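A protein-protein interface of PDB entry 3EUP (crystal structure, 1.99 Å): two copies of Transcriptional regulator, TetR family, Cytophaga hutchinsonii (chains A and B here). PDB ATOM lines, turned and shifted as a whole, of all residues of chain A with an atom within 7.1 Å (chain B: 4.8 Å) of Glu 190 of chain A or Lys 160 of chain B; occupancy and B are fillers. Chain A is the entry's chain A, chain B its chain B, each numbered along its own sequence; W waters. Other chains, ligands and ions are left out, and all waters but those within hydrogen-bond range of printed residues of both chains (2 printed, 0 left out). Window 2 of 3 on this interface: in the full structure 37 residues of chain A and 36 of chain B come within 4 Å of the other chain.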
ATOM      1  N   SER A  92     -32.297 -16.862 -10.763  1.00  0.00           N
ATOM      2  CA  SER A  92     -31.143 -17.522 -11.335  1.00  0.00           C
ATOM      3  C   SER A  92     -31.393 -18.997 -11.711  1.00  0.00           C
ATOM      4  O   SER A  92     -30.967 -19.463 -12.776  1.00  0.00           O
ATOM      5  CB  SER A  92     -29.951 -17.476 -10.398  1.00  0.00           C
ATOM      6  OG  SER A  92     -28.891 -18.093 -11.069  1.00  0.00           O
ATOM      7  N   LEU A 168     -32.706  -5.964 -12.489  1.00  0.00           N
ATOM      8  CA  LEU A 168     -31.561  -6.825 -12.392  1.00  0.00           C
ATOM      9  C   LEU A 168     -31.747  -8.158 -13.116  1.00  0.00           C
ATOM     10  O   LEU A 168     -30.802  -8.644 -13.739  1.00  0.00           O
ATOM     11  CB  LEU A 168     -31.186  -7.061 -10.940  1.00  0.00           C
ATOM     12  CG  LEU A 168     -30.448  -5.929 -10.219  1.00  0.00           C
ATOM     13  CD1 LEU A 168     -30.360  -6.272  -8.692  1.00  0.00           C
ATOM     14  CD2 LEU A 168     -29.085  -5.704 -10.855  1.00  0.00           C
ATOM     15  N   TYR A 184     -21.001 -13.976 -17.056  1.00  0.00           N
ATOM     16  CA  TYR A 184     -21.171 -12.539 -16.956  1.00  0.00           C
ATOM     17  C   TYR A 184     -22.514 -12.240 -16.303  1.00  0.00           C
ATOM     18  O   TYR A 184     -22.592 -11.365 -15.462  1.00  0.00           O
ATOM     19  CB  TYR A 184     -21.063 -11.867 -18.319  1.00  0.00           C
ATOM     20  CG  TYR A 184     -19.747 -12.056 -19.013  1.00  0.00           C
ATOM     21  CD1 TYR A 184     -18.538 -12.140 -18.314  1.00  0.00           C
ATOM     22  CD2 TYR A 184     -19.705 -12.129 -20.379  1.00  0.00           C
ATOM     23  CE1 TYR A 184     -17.333 -12.310 -18.991  1.00  0.00           C
ATOM     24  CE2 TYR A 184     -18.510 -12.307 -21.049  1.00  0.00           C
ATOM     25  CZ  TYR A 184     -17.344 -12.381 -20.366  1.00  0.00           C
ATOM     26  OH  TYR A 184     -16.206 -12.524 -21.121  1.00  0.00           O
ATOM     27  N   SER A 185     -23.575 -12.927 -16.724  1.00  0.00           N
ATOM     28  CA  SER A 185     -24.877 -12.703 -16.113  1.00  0.00           C
ATOM     29  C   SER A 185     -24.866 -13.198 -14.657  1.00  0.00           C
ATOM     30  O   SER A 185     -25.581 -12.645 -13.813  1.00  0.00           O
ATOM     31  CB  SER A 185     -25.995 -13.334 -16.950  1.00  0.00           C
ATOM     32  OG  SER A 185     -25.648 -14.661 -17.376  1.00  0.00           O
ATOM     33  N   ASP A 186     -24.057 -14.222 -14.330  1.00  0.00           N
ATOM     34  CA  ASP A 186     -23.956 -14.686 -12.913  1.00  0.00           C
ATOM     35  C   ASP A 186     -23.547 -13.544 -11.961  1.00  0.00           C
ATOM     36  O   ASP A 186     -23.976 -13.516 -10.823  1.00  0.00           O
ATOM     37  CB  ASP A 186     -22.982 -15.881 -12.744  1.00  0.00           C
ATOM     38  CG  ASP A 186     -23.557 -17.173 -13.252  1.00  0.00           C
ATOM     39  OD1 ASP A 186     -24.794 -17.230 -13.476  1.00  0.00           O
ATOM     40  OD2 ASP A 186     -22.756 -18.098 -13.516  1.00  0.00           O
ATOM     41  N   TYR A 187     -22.743 -12.591 -12.425  1.00  0.00           N
ATOM     42  CA  TYR A 187     -22.409 -11.424 -11.582  1.00  0.00           C
ATOM     43  C   TYR A 187     -23.651 -10.588 -11.228  1.00  0.00           C
ATOM     44  O   TYR A 187     -23.783 -10.114 -10.098  1.00  0.00           O
ATOM     45  CB  TYR A 187     -21.372 -10.500 -12.219  1.00  0.00           C
ATOM     46  CG  TYR A 187     -20.003 -11.086 -12.324  1.00  0.00           C
ATOM     47  CD1 TYR A 187     -19.214 -11.324 -11.183  1.00  0.00           C
ATOM     48  CD2 TYR A 187     -19.463 -11.380 -13.561  1.00  0.00           C
ATOM     49  CE1 TYR A 187     -17.939 -11.847 -11.301  1.00  0.00           C
ATOM     50  CE2 TYR A 187     -18.194 -11.900 -13.683  1.00  0.00           C
ATOM     51  CZ  TYR A 187     -17.443 -12.143 -12.547  1.00  0.00           C
ATOM     52  OH  TYR A 187     -16.186 -12.662 -12.687  1.00  0.00           O
ATOM     53  N   VAL A 188     -24.604 -10.505 -12.142  1.00  0.00           N
ATOM     54  CA  VAL A 188     -25.821  -9.714 -11.881  1.00  0.00           C
ATOM     55  C   VAL A 188     -26.755 -10.438 -10.895  1.00  0.00           C
ATOM     56  O   VAL A 188     -27.394  -9.818 -10.001  1.00  0.00           O
ATOM     57  CB  VAL A 188     -26.517  -9.374 -13.202  1.00  0.00           C
ATOM     58  CG1 VAL A 188     -27.769  -8.449 -12.971  1.00  0.00           C
ATOM     59  CG2 VAL A 188     -25.484  -8.739 -14.169  1.00  0.00           C
ATOM     60  N   PHE A 189     -26.872 -11.751 -11.060  1.00  0.00           N
ATOM     61  CA  PHE A 189     -27.667 -12.535 -10.122  1.00  0.00           C
ATOM     62  C   PHE A 189     -27.057 -12.454  -8.731  1.00  0.00           C
ATOM     63  O   PHE A 189     -27.787 -12.478  -7.715  1.00  0.00           O
ATOM     64  CB  PHE A 189     -27.791 -13.991 -10.623  1.00  0.00           C
ATOM     65  CG  PHE A 189     -28.755 -14.129 -11.760  1.00  0.00           C
ATOM     66  CD1 PHE A 189     -30.101 -13.850 -11.551  1.00  0.00           C
ATOM     67  CD2 PHE A 189     -28.358 -14.499 -13.020  1.00  0.00           C
ATOM     68  CE1 PHE A 189     -31.017 -13.924 -12.583  1.00  0.00           C
ATOM     69  CE2 PHE A 189     -29.272 -14.601 -14.044  1.00  0.00           C
ATOM     70  CZ  PHE A 189     -30.635 -14.307 -13.812  1.00  0.00           C
ATOM     71  N   GLU A 190     -25.732 -12.363  -8.678  1.00  0.00           N
ATOM     72  CA  GLU A 190     -25.043 -12.163  -7.412  1.00  0.00           C
ATOM     73  C   GLU A 190     -25.456 -10.808  -6.775  1.00  0.00           C
ATOM     74  O   GLU A 190     -25.718 -10.718  -5.559  1.00  0.00           O
ATOM     75  CB  GLU A 190     -23.521 -12.243  -7.630  1.00  0.00           C
ATOM     76  CG  GLU A 190     -22.769 -12.655  -6.453  1.00  0.00           C
ATOM     77  CD  GLU A 190     -21.251 -12.430  -6.609  1.00  0.00           C
ATOM     78  OE1 GLU A 190     -20.719 -12.575  -7.759  1.00  0.00           O
ATOM     79  OE2 GLU A 190     -20.619 -12.061  -5.572  1.00  0.00           O
ATOM     80  N   SER A 191     -25.533  -9.758  -7.582  1.00  0.00           N
ATOM     81  CA  SER A 191     -26.034  -8.498  -7.073  1.00  0.00           C
ATOM     82  C   SER A 191     -27.516  -8.568  -6.714  1.00  0.00           C
ATOM     83  O   SER A 191     -27.921  -7.864  -5.860  1.00  0.00           O
ATOM     84  CB  SER A 191     -25.771  -7.343  -8.062  1.00  0.00           C
ATOM     85  OG  SER A 191     -24.375  -7.028  -8.116  1.00  0.00           O
ATOM     86  N   LEU A 192     -28.337  -9.367  -7.379  1.00  0.00           N
ATOM     87  CA  LEU A 192     -29.706  -9.538  -6.901  1.00  0.00           C
ATOM     88  C   LEU A 192     -29.707 -10.080  -5.460  1.00  0.00           C
ATOM     89  O   LEU A 192     -30.432  -9.583  -4.603  1.00  0.00           O
ATOM     90  CB  LEU A 192     -30.471 -10.487  -7.793  1.00  0.00           C
ATOM     91  CG  LEU A 192     -31.938 -10.756  -7.502  1.00  0.00           C
ATOM     92  CD1 LEU A 192     -32.810  -9.467  -7.635  1.00  0.00           C
ATOM     93  CD2 LEU A 192     -32.394 -11.805  -8.488  1.00  0.00           C
ATOM     94  N   GLU A 193     -28.904 -11.098  -5.195  1.00  0.00           N
ATOM     95  CA  GLU A 193     -28.752 -11.584  -3.823  1.00  0.00           C
ATOM     96  C   GLU A 193     -28.310 -10.494  -2.844  1.00  0.00           C
ATOM     97  O   GLU A 193     -28.842 -10.389  -1.743  1.00  0.00           O
ATOM     98  CB  GLU A 193     -27.720 -12.711  -3.761  1.00  0.00           C
ATOM     99  CG  GLU A 193     -28.230 -14.032  -4.220  1.00  0.00           C
ATOM    100  CD  GLU A 193     -27.675 -15.199  -3.386  1.00  0.00           C
ATOM    101  OE1 GLU A 193     -26.652 -15.004  -2.691  1.00  0.00           O
ATOM    102  OE2 GLU A 193     -28.272 -16.306  -3.426  1.00  0.00           O
ATOM    103  N   ASP A 194     -27.311  -9.707  -3.220  1.00  0.00           N
ATOM    104  CA  ASP A 194     -26.867  -8.589  -2.371  1.00  0.00           C
ATOM    105  C   ASP A 194     -28.020  -7.583  -2.082  1.00  0.00           C
ATOM    106  O   ASP A 194     -28.149  -7.081  -0.969  1.00  0.00           O
ATOM    107  CB  ASP A 194     -25.688  -7.845  -3.013  1.00  0.00           C
ATOM    108  CG  ASP A 194     -24.479  -8.754  -3.255  1.00  0.00           C
ATOM    109  OD1 ASP A 194     -24.340  -9.763  -2.528  1.00  0.00           O
ATOM    110  OD2 ASP A 194     -23.658  -8.472  -4.163  1.00  0.00           O
ATOM    111  N   LEU A 195     -28.851  -7.287  -3.075  1.00  0.00           N
ATOM    112  CA  LEU A 195     -29.951  -6.354  -2.856  1.00  0.00           C
ATOM    113  C   LEU A 195     -30.858  -6.855  -1.737  1.00  0.00           C
ATOM    114  O   LEU A 195     -31.210  -6.116  -0.831  1.00  0.00           O
ATOM    115  CB  LEU A 195     -30.764  -6.148  -4.157  1.00  0.00           C
ATOM    116  CG  LEU A 195     -31.914  -5.153  -4.204  1.00  0.00           C
ATOM    117  CD1 LEU A 195     -31.389  -3.700  -4.032  1.00  0.00           C
ATOM    118  CD2 LEU A 195     -32.670  -5.286  -5.506  1.00  0.00           C
ATOM    119  N   ASP B 157     -15.557  -5.428  -5.599  1.00  0.00           N
ATOM    120  CA  ASP B 157     -15.620  -6.454  -6.631  1.00  0.00           C
ATOM    121  C   ASP B 157     -15.988  -5.759  -7.966  1.00  0.00           C
ATOM    122  O   ASP B 157     -17.168  -5.589  -8.317  1.00  0.00           O
ATOM    123  CB  ASP B 157     -16.622  -7.546  -6.274  1.00  0.00           C
ATOM    124  CG  ASP B 157     -16.639  -8.682  -7.280  1.00  0.00           C
ATOM    125  OD1 ASP B 157     -16.142  -8.541  -8.442  1.00  0.00           O
ATOM    126  OD2 ASP B 157     -17.198  -9.731  -6.895  1.00  0.00           O
ATOM    127  N   VAL B 158     -14.938  -5.347  -8.678  1.00  0.00           N
ATOM    128  CA  VAL B 158     -15.078  -4.356  -9.769  1.00  0.00           C
ATOM    129  C   VAL B 158     -15.911  -4.913 -10.883  1.00  0.00           C
ATOM    130  O   VAL B 158     -16.719  -4.208 -11.478  1.00  0.00           O
ATOM    131  CB  VAL B 158     -13.690  -3.893 -10.299  1.00  0.00           C
ATOM    132  CG1 VAL B 158     -13.854  -2.913 -11.459  1.00  0.00           C
ATOM    133  CG2 VAL B 158     -12.880  -3.225  -9.156  1.00  0.00           C
ATOM    134  N   THR B 159     -15.692  -6.192 -11.181  1.00  0.00           N
ATOM    135  CA  THR B 159     -16.377  -6.823 -12.287  1.00  0.00           C
ATOM    136  C   THR B 159     -17.835  -6.950 -11.970  1.00  0.00           C
ATOM    137  O   THR B 159     -18.680  -6.600 -12.797  1.00  0.00           O
ATOM    138  CB  THR B 159     -15.681  -8.176 -12.650  1.00  0.00           C
ATOM    139  OG1 THR B 159     -14.421  -7.848 -13.255  1.00  0.00           O
ATOM    140  CG2 THR B 159     -16.497  -9.039 -13.630  1.00  0.00           C
ATOM    141  N   LYS B 160     -18.150  -7.370 -10.748  1.00  0.00           N
ATOM    142  CA  LYS B 160     -19.528  -7.530 -10.373  1.00  0.00           C
ATOM    143  C   LYS B 160     -20.244  -6.181 -10.455  1.00  0.00           C
ATOM    144  O   LYS B 160     -21.363  -6.097 -10.969  1.00  0.00           O
ATOM    145  CB  LYS B 160     -19.659  -8.127  -8.970  1.00  0.00           C
ATOM    146  CG  LYS B 160     -21.101  -8.143  -8.450  1.00  0.00           C
ATOM    147  CD  LYS B 160     -21.213  -8.918  -7.134  1.00  0.00           C
ATOM    148  CE  LYS B 160     -20.789  -8.102  -5.969  1.00  0.00           C
ATOM    149  NZ  LYS B 160     -21.183  -8.878  -4.744  1.00  0.00           N
ATOM    150  N   ILE B 161     -19.607  -5.127  -9.955  1.00  0.00           N
ATOM    151  CA  ILE B 161     -20.265  -3.834  -9.983  1.00  0.00           C
ATOM    152  C   ILE B 161     -20.487  -3.370 -11.456  1.00  0.00           C
ATOM    153  O   ILE B 161     -21.560  -2.889 -11.804  1.00  0.00           O
ATOM    154  CB  ILE B 161     -19.472  -2.792  -9.154  1.00  0.00           C
ATOM    155  CG1 ILE B 161     -19.407  -3.227  -7.677  1.00  0.00           C
ATOM    156  CG2 ILE B 161     -20.041  -1.338  -9.344  1.00  0.00           C
ATOM    157  CD1 ILE B 161     -20.659  -3.001  -6.818  1.00  0.00           C
ATOM    158  N   ALA B 162     -19.481  -3.542 -12.311  1.00  0.00           N
ATOM    159  CA  ALA B 162     -19.575  -3.064 -13.682  1.00  0.00           C
ATOM    160  C   ALA B 162     -20.745  -3.759 -14.398  1.00  0.00           C
ATOM    161  O   ALA B 162     -21.643  -3.106 -14.955  1.00  0.00           O
ATOM    162  CB  ALA B 162     -18.205  -3.294 -14.408  1.00  0.00           C
ATOM    163  N   PHE B 163     -20.780  -5.080 -14.348  1.00  0.00           N
ATOM    164  CA  PHE B 163     -21.881  -5.773 -14.970  1.00  0.00           C
ATOM    165  C   PHE B 163     -23.212  -5.402 -14.349  1.00  0.00           C
ATOM    166  O   PHE B 163     -24.189  -5.312 -15.093  1.00  0.00           O
ATOM    167  CB  PHE B 163     -21.700  -7.295 -14.985  1.00  0.00           C
ATOM    168  CG  PHE B 163     -20.765  -7.769 -16.046  1.00  0.00           C
ATOM    169  CD1 PHE B 163     -21.067  -7.556 -17.402  1.00  0.00           C
ATOM    170  CD2 PHE B 163     -19.581  -8.420 -15.712  1.00  0.00           C
ATOM    171  CE1 PHE B 163     -20.195  -8.003 -18.411  1.00  0.00           C
ATOM    172  CE2 PHE B 163     -18.687  -8.859 -16.735  1.00  0.00           C
ATOM    173  CZ  PHE B 163     -18.984  -8.641 -18.073  1.00  0.00           C
ATOM    174  N   SER B 164     -23.228  -5.166 -13.023  1.00  0.00           N
ATOM    175  CA  SER B 164     -24.472  -4.850 -12.308  1.00  0.00           C
ATOM    176  C   SER B 164     -24.995  -3.458 -12.714  1.00  0.00           C
ATOM    177  O   SER B 164     -26.213  -3.274 -12.847  1.00  0.00           O
ATOM    178  CB  SER B 164     -24.333  -5.036 -10.789  1.00  0.00           C
ATOM    179  OG  SER B 164     -24.068  -6.428 -10.519  1.00  0.00           O
HETATM  180  O   HOH W   1     -18.206 -12.031  -7.695  1.00  0.00           O
HETATM  181  O   HOH W   2     -18.371 -10.119  -4.611  1.00  0.00           O
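Water W1 lies within hydrogen-bond range of the side-chain carboxylate (OE1) of Glu 190 of chain A (2.6 Å) and the side-chain carboxylate (OD2) of Asp 157 of chain B (2.6 Å). Water W2 lies within hydrogen-bond range of the side-chain carboxylate of Asp 157 of chain B, the side-chain amino group of Lys 160 of chain B and the side-chain carboxylate of Glu 190 of chain A.
N of Lys 160 of chain B sits at hydrogen-bond distance from OD1 of Asp 157 of chain B (3.3 Å). The backbone carbonyl oxygen (O) of Lys 160 of chain B lies within hydrogen-bond range of the side-chain hydroxyl (OG) of Ser 164 of chain B (2.8 Å).
Hydrophobic or aromatic side chains of chain B within 4 Å of the printed part of chain A: Phe 163. Hydrophobic or aromatic side chains of chain A within 4 Å of the printed part of chain B: Tyr 184, Tyr 187 and Val 188. Among the printed residues, 11 pairs touch across the chains. Among the printed residues, Asp or Glu carboxylates within 4 Å of a Lys or Arg side-chain nitrogen of the other chain: Glu 190 of chain A with Lys 160 of chain B and Asp 194 of chain A with Lys 160 of chain B.
Among the printed residues, pairs that only touch across the chains: Tyr 184 of chain A with Phe 163 of chain B, Tyr 187 of chain A with Thr 159 of chain B, Tyr 187 of chain A with Lys 160 of chain B, Tyr 187 of chain A with Phe 163 of chain B, Tyr 187 of chain A with Ser 164 of chain B, Val 188 of chain A with Phe 163 of chain B, Val 188 of chain A with Ser 164 of chain B and Ser 191 of chain A with Lys 160 of chain B.
The side-chain amino group (NZ) of Lys 160 of chain B lies within salt-bridge range of the side-chain carboxylate (OE2) of Glu 190 of chain A, at 3.3 Å. The side-chain hydroxyl (OG) of Ser 191 of chain A is in hydrogen-bond range of the side-chain hydroxyl (OG) of Ser 164 of chain B, at 2.5 Å. NZ of Lys 160 of chain B is in salt-bridge range of OD2 of Asp 194 of chain A, 2.6 Å away.
No position is printed for both chains. Of the 11 pairs that touch across the chains among the printed residues, none has its exchanged pair printed and touching as well.
Of chain B, only Lys 160 comes within 4 Å of Glu 190 of chain A. Of the printed residues of chain B, Asp 194 of chain A touches Lys 160 (2.6 Å). Leu 195 of chain A touches none of the printed residues of chain B. Of the printed residues of chain A, Thr 159 of chain B touches Tyr 187 (3.3 Å). Lys 160 of chain B touches just these residues of chain A: Tyr 187, Glu 190, Ser 191 and Asp 194. The nearest residue of chain B that does not touch Glu 190 of chain A is Asp 157 of chain B (4.3 Å). The nearest residue of chain A that does not touch Lys 160 of chain B is Val 188 of chain A (5.6 Å).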
